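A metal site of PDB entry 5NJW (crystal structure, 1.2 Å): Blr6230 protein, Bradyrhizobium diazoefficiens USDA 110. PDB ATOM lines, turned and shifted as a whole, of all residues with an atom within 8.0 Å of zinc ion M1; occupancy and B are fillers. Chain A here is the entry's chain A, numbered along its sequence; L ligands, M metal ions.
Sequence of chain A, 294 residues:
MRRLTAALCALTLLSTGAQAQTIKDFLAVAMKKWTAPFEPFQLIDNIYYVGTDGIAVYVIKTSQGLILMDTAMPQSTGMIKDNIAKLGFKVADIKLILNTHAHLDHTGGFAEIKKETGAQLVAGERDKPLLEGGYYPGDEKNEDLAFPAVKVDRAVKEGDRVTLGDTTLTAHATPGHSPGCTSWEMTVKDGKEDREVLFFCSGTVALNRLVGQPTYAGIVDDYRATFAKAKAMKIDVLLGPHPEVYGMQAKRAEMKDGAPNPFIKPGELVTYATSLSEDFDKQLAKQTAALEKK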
ATOM      1  N   PHE A  26      17.428 -20.561  -4.422  1.00  0.00           N
ATOM      2  CA  PHE A  26      17.840 -21.035  -5.747  1.00  0.00           C
ATOM      3  C   PHE A  26      18.051 -22.561  -5.716  1.00  0.00           C
ATOM      4  O   PHE A  26      17.543 -23.298  -6.612  1.00  0.00           O
ATOM      5  CB  PHE A  26      19.102 -20.310  -6.229  1.00  0.00           C
ATOM      6  CG  PHE A  26      19.651 -20.821  -7.533  1.00  0.00           C
ATOM      7  CD1 PHE A  26      19.230 -20.301  -8.746  1.00  0.00           C
ATOM      8  CD2 PHE A  26      20.605 -21.826  -7.545  1.00  0.00           C
ATOM      9  CE1 PHE A  26      19.733 -20.789  -9.950  1.00  0.00           C
ATOM     10  CE2 PHE A  26      21.124 -22.321  -8.738  1.00  0.00           C
ATOM     11  CZ  PHE A  26      20.687 -21.790  -9.940  1.00  0.00           C
ATOM     12  N   TRP A  34      13.121 -28.123 -10.737  1.00  0.00           N
ATOM     13  CA  TRP A  34      13.999 -28.243 -11.910  1.00  0.00           C
ATOM     14  C   TRP A  34      14.496 -29.651 -12.230  1.00  0.00           C
ATOM     15  O   TRP A  34      15.057 -29.876 -13.300  1.00  0.00           O
ATOM     16  CB  TRP A  34      15.180 -27.284 -11.746  1.00  0.00           C
ATOM     17  CG  TRP A  34      14.794 -25.821 -11.821  1.00  0.00           C
ATOM     18  CD1 TRP A  34      13.524 -25.286 -11.895  1.00  0.00           C
ATOM     19  CD2 TRP A  34      15.677 -24.712 -11.785  1.00  0.00           C
ATOM     20  NE1 TRP A  34      13.597 -23.918 -11.934  1.00  0.00           N
ATOM     21  CE2 TRP A  34      14.901 -23.540 -11.897  1.00  0.00           C
ATOM     22  CE3 TRP A  34      17.052 -24.585 -11.705  1.00  0.00           C
ATOM     23  CZ2 TRP A  34      15.470 -22.260 -11.875  1.00  0.00           C
ATOM     24  CZ3 TRP A  34      17.608 -23.310 -11.686  1.00  0.00           C
ATOM     25  CH2 TRP A  34      16.817 -22.190 -11.806  1.00  0.00           C
ATOM     26  N   GLY A  54      11.610 -27.703 -15.456  1.00  0.00           N
ATOM     27  CA  GLY A  54      12.153 -26.398 -15.096  1.00  0.00           C
ATOM     28  C   GLY A  54      13.421 -25.927 -15.782  1.00  0.00           C
ATOM     29  O   GLY A  54      13.779 -24.758 -15.628  1.00  0.00           O
ATOM     30  N   ILE A  55      14.113 -26.794 -16.513  1.00  0.00           N
ATOM     31  CA  ILE A  55      15.360 -26.461 -17.252  1.00  0.00           C
ATOM     32  C   ILE A  55      15.177 -26.985 -18.670  1.00  0.00           C
ATOM     33  O   ILE A  55      14.882 -28.153 -18.879  1.00  0.00           O
ATOM     34  CB  ILE A  55      16.604 -27.074 -16.600  1.00  0.00           C
ATOM     35  CG1 ILE A  55      16.845 -26.479 -15.188  1.00  0.00           C
ATOM     36  CG2 ILE A  55      17.812 -26.859 -17.507  1.00  0.00           C
ATOM     37  CD1 ILE A  55      17.852 -27.276 -14.371  1.00  0.00           C
ATOM     38  N   ALA A  56      15.387 -26.102 -19.632  1.00  0.00           N
ATOM     39  CA  ALA A  56      15.206 -26.486 -21.042  1.00  0.00           C
ATOM     40  C   ALA A  56      16.499 -26.942 -21.655  1.00  0.00           C
ATOM     41  O   ALA A  56      17.536 -26.272 -21.533  1.00  0.00           O
ATOM     42  CB  ALA A  56      14.674 -25.292 -21.806  1.00  0.00           C
ATOM     43  N   MET A  73      20.920 -29.786 -14.270  1.00  0.00           N
ATOM     44  CA  MET A  73      21.697 -29.870 -13.031  1.00  0.00           C
ATOM     45  C   MET A  73      22.619 -31.092 -13.054  1.00  0.00           C
ATOM     46  O   MET A  73      22.318 -32.077 -13.747  1.00  0.00           O
ATOM     47  CB  MET A  73      20.769 -29.967 -11.805  1.00  0.00           C
ATOM     48  CG  MET A  73      19.984 -28.706 -11.506  1.00  0.00           C
ATOM     49  SD  MET A  73      21.035 -27.381 -10.865  1.00  0.00           S
ATOM     50  CE  MET A  73      21.348 -27.968  -9.191  1.00  0.00           C
ATOM     51  N   THR A 100      24.484 -22.011 -23.754  1.00  0.00           N
ATOM     52  CA  THR A 100      23.969 -20.647 -23.699  1.00  0.00           C
ATOM     53  C   THR A 100      24.773 -19.859 -22.662  1.00  0.00           C
ATOM     54  O   THR A 100      25.335 -18.803 -22.959  1.00  0.00           O
ATOM     55  CB  THR A 100      22.483 -20.603 -23.299  1.00  0.00           C
ATOM     56  OG1 THR A 100      22.266 -21.405 -22.126  1.00  0.00           O
ATOM     57  CG2 THR A 100      21.600 -21.044 -24.441  1.00  0.00           C
ATOM     58  N   HIS A 101      24.887 -20.378 -21.427  1.00  0.00           N
ATOM     59  CA  HIS A 101      25.703 -19.709 -20.424  1.00  0.00           C
ATOM     60  C   HIS A 101      26.125 -20.694 -19.329  1.00  0.00           C
ATOM     61  O   HIS A 101      25.487 -21.729 -19.078  1.00  0.00           O
ATOM     62  CB  HIS A 101      24.972 -18.506 -19.807  1.00  0.00           C
ATOM     63  CG  HIS A 101      23.871 -18.862 -18.844  1.00  0.00           C
ATOM     64  ND1 HIS A 101      22.551 -18.981 -19.190  1.00  0.00           N
ATOM     65  CD2 HIS A 101      23.912 -19.067 -17.514  1.00  0.00           C
ATOM     66  CE1 HIS A 101      21.822 -19.255 -18.123  1.00  0.00           C
ATOM     67  NE2 HIS A 101      22.635 -19.343 -17.093  1.00  0.00           N
ATOM     68  N   HIS A 103      26.363 -21.602 -16.073  1.00  0.00           N
ATOM     69  CA  HIS A 103      25.914 -21.897 -14.695  1.00  0.00           C
ATOM     70  C   HIS A 103      25.538 -23.353 -14.543  1.00  0.00           C
ATOM     71  O   HIS A 103      25.110 -23.982 -15.547  1.00  0.00           O
ATOM     72  CB  HIS A 103      24.708 -21.040 -14.324  1.00  0.00           C
ATOM     73  CG  HIS A 103      25.001 -19.587 -14.202  1.00  0.00           C
ATOM     74  ND1 HIS A 103      24.009 -18.632 -14.316  1.00  0.00           N
ATOM     75  CD2 HIS A 103      26.146 -18.920 -13.918  1.00  0.00           C
ATOM     76  CE1 HIS A 103      24.531 -17.439 -14.107  1.00  0.00           C
ATOM     77  NE2 HIS A 103      25.823 -17.576 -13.895  1.00  0.00           N
ATOM     78  N   LEU A 104      25.664 -23.884 -13.333  1.00  0.00           N
ATOM     79  CA  LEU A 104      25.512 -25.317 -13.084  1.00  0.00           C
ATOM     80  C   LEU A 104      24.191 -25.921 -13.540  1.00  0.00           C
ATOM     81  O   LEU A 104      24.151 -27.103 -13.813  1.00  0.00           O
ATOM     82  CB  LEU A 104      25.740 -25.677 -11.616  1.00  0.00           C
ATOM     83  CG  LEU A 104      24.619 -25.461 -10.629  1.00  0.00           C
ATOM     84  CD1 LEU A 104      24.929 -26.252  -9.342  1.00  0.00           C
ATOM     85  CD2 LEU A 104      24.416 -23.974 -10.374  1.00  0.00           C
ATOM     86  N   ASP A 105      23.115 -25.141 -13.541  1.00  0.00           N
ATOM     87  CA  ASP A 105      21.836 -25.659 -13.970  1.00  0.00           C
ATOM     88  C   ASP A 105      21.759 -25.892 -15.497  1.00  0.00           C
ATOM     89  O   ASP A 105      20.791 -26.476 -15.975  1.00  0.00           O
ATOM     90  CB  ASP A 105      20.673 -24.807 -13.456  1.00  0.00           C
ATOM     91  CG  ASP A 105      20.765 -23.316 -13.808  1.00  0.00           C
ATOM     92  OD1 ASP A 105      21.856 -22.712 -13.750  1.00  0.00           O
ATOM     93  OD2 ASP A 105      19.674 -22.739 -14.105  1.00  0.00           O
ATOM     94  N   HIS A 106      22.765 -25.430 -16.255  1.00  0.00           N
ATOM     95  CA  HIS A 106      22.855 -25.646 -17.699  1.00  0.00           C
ATOM     96  C   HIS A 106      24.086 -26.440 -18.087  1.00  0.00           C
ATOM     97  O   HIS A 106      24.133 -26.981 -19.194  1.00  0.00           O
ATOM     98  CB  HIS A 106      22.803 -24.328 -18.436  1.00  0.00           C
ATOM     99  CG  HIS A 106      21.662 -23.512 -17.978  1.00  0.00           C
ATOM    100  ND1 HIS A 106      20.356 -23.861 -18.223  1.00  0.00           N
ATOM    101  CD2 HIS A 106      21.613 -22.419 -17.190  1.00  0.00           C
ATOM    102  CE1 HIS A 106      19.553 -23.022 -17.591  1.00  0.00           C
ATOM    103  NE2 HIS A 106      20.296 -22.112 -16.976  1.00  0.00           N
ATOM    104  N   HIS A 177      23.729 -11.933 -17.796  1.00  0.00           N
ATOM    105  CA  HIS A 177      23.443 -13.030 -16.891  1.00  0.00           C
ATOM    106  C   HIS A 177      24.722 -13.831 -16.616  1.00  0.00           C
ATOM    107  O   HIS A 177      24.925 -14.345 -15.509  1.00  0.00           O
ATOM    108  CB  HIS A 177      22.304 -13.861 -17.455  1.00  0.00           C
ATOM    109  CG  HIS A 177      21.893 -14.986 -16.573  1.00  0.00           C
ATOM    110  ND1 HIS A 177      21.043 -14.845 -15.505  1.00  0.00           N
ATOM    111  CD2 HIS A 177      22.286 -16.270 -16.567  1.00  0.00           C
ATOM    112  CE1 HIS A 177      20.868 -16.011 -14.923  1.00  0.00           C
ATOM    113  NE2 HIS A 177      21.642 -16.897 -15.523  1.00  0.00           N
ATOM    114  N   CYS A 201      19.928 -16.675 -24.274  1.00  0.00           N
ATOM    115  CA  CYS A 201      20.792 -17.247 -23.258  1.00  0.00           C
ATOM    116  C   CYS A 201      20.350 -17.085 -21.836  1.00  0.00           C
ATOM    117  O   CYS A 201      20.885 -17.777 -20.993  1.00  0.00           O
ATOM    118  CB  CYS A 201      22.209 -16.727 -23.414  1.00  0.00           C
ATOM    119  SG  CYS A 201      22.473 -15.047 -22.881  1.00  0.00           S
ATOM    120  N   SER A 202      19.440 -16.149 -21.590  1.00  0.00           N
ATOM    121  CA  SER A 202      18.949 -15.678 -20.265  1.00  0.00           C
ATOM    122  C   SER A 202      19.330 -14.231 -20.049  1.00  0.00           C
ATOM    123  O   SER A 202      20.497 -13.847 -20.297  1.00  0.00           O
ATOM    124  CB  SER A 202      19.483 -16.391 -19.015  1.00  0.00           C
ATOM    125  OG  SER A 202      19.008 -15.696 -17.859  1.00  0.00           O
ATOM    126  N   THR A 204      17.967 -12.716 -16.874  1.00  0.00           N
ATOM    127  CA  THR A 204      17.523 -12.494 -15.506  1.00  0.00           C
ATOM    128  C   THR A 204      18.711 -12.033 -14.637  1.00  0.00           C
ATOM    129  O   THR A 204      19.860 -12.341 -14.907  1.00  0.00           O
ATOM    130  CB  THR A 204      16.941 -13.792 -14.913  1.00  0.00           C
ATOM    131  OG1 THR A 204      17.987 -14.751 -14.843  1.00  0.00           O
ATOM    132  CG2 THR A 204      15.769 -14.300 -15.740  1.00  0.00           C
ATOM    133  N   ALA A 206      18.795 -12.839 -11.238  1.00  0.00           N
ATOM    134  CA  ALA A 206      18.984 -14.083 -10.507  1.00  0.00           C
ATOM    135  C   ALA A 206      19.951 -13.867  -9.328  1.00  0.00           C
ATOM    136  O   ALA A 206      19.652 -12.985  -8.488  1.00  0.00           O
ATOM    137  CB  ALA A 206      19.380 -15.183 -11.475  1.00  0.00           C
ATOM    138  N   PRO A 241      16.794 -21.078 -21.861  1.00  0.00           N
ATOM    139  CA  PRO A 241      17.349 -22.184 -21.056  1.00  0.00           C
ATOM    140  C   PRO A 241      16.450 -22.628 -19.918  1.00  0.00           C
ATOM    141  O   PRO A 241      16.792 -23.596 -19.242  1.00  0.00           O
ATOM    142  CB  PRO A 241      18.657 -21.611 -20.506  1.00  0.00           C
ATOM    143  CG  PRO A 241      18.651 -20.210 -20.767  1.00  0.00           C
ATOM    144  CD  PRO A 241      17.497 -19.814 -21.611  1.00  0.00           C
ATOM    145  N   HIS A 242      15.343 -21.924 -19.693  1.00  0.00           N
ATOM    146  CA  HIS A 242      14.291 -22.355 -18.792  1.00  0.00           C
ATOM    147  C   HIS A 242      12.981 -22.218 -19.565  1.00  0.00           C
ATOM    148  O   HIS A 242      12.809 -21.251 -20.303  1.00  0.00           O
ATOM    149  CB  HIS A 242      14.273 -21.483 -17.524  1.00  0.00           C
ATOM    150  CG  HIS A 242      15.494 -21.635 -16.665  1.00  0.00           C
ATOM    151  ND1 HIS A 242      15.674 -22.697 -15.807  1.00  0.00           N
ATOM    152  CD2 HIS A 242      16.612 -20.889 -16.577  1.00  0.00           C
ATOM    153  CE1 HIS A 242      16.849 -22.600 -15.219  1.00  0.00           C
ATOM    154  NE2 HIS A 242      17.437 -21.507 -15.665  1.00  0.00           N
HETATM  155  O1  LIG L   1      21.000 -20.147 -14.359  1.00  0.00           O
HETATM  156  B1  LG2 L   2      18.416 -18.278 -15.275  1.00  0.00           B
HETATM  157  O1  LG2 L   2      19.263 -19.184 -16.167  1.00  0.00           O
HETATM  158  O2  LG2 L   2      18.120 -18.689 -13.818  1.00  0.00           O
HETATM  159  O3  LG2 L   2      17.780 -17.000 -15.852  1.00  0.00           O
HETATM  160 ZN    ZN M   1      19.498 -21.066 -15.368  1.00  0.00          ZN
HETATM  161 ZN    ZN M   2      22.091 -18.882 -15.163  1.00  0.00          ZN
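NE2 of His 101 touches zinc ion M1 (3.97 Å).
Four residues have an atom within 4 Å of zinc ion M1: His 101, Asp 105, His 106 and His 242.
The backbone carbonyl oxygen (O) of Gly 54 is in hydrogen-bond range of a ring nitrogen (ND1) of His 242.
A ring nitrogen (ND1) of His 101 is in hydrogen-bond range of the backbone carbonyl oxygen of Cys 201 (2.7 Å).
O1 of LIG L1 binds zinc ion M1.
Zinc ion M1 is bound by O1 of LG2 L2, at 2.1 Å.
Zinc ion M1 is bound by NE2 of His 106 (2.1 Å).
The side-chain carboxylate (OD2) of Asp 105 binds zinc ion M1, at 2.1 Å.
Zinc ion M1 is bound by a ring nitrogen (NE2) of His 242 (2.1 Å).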
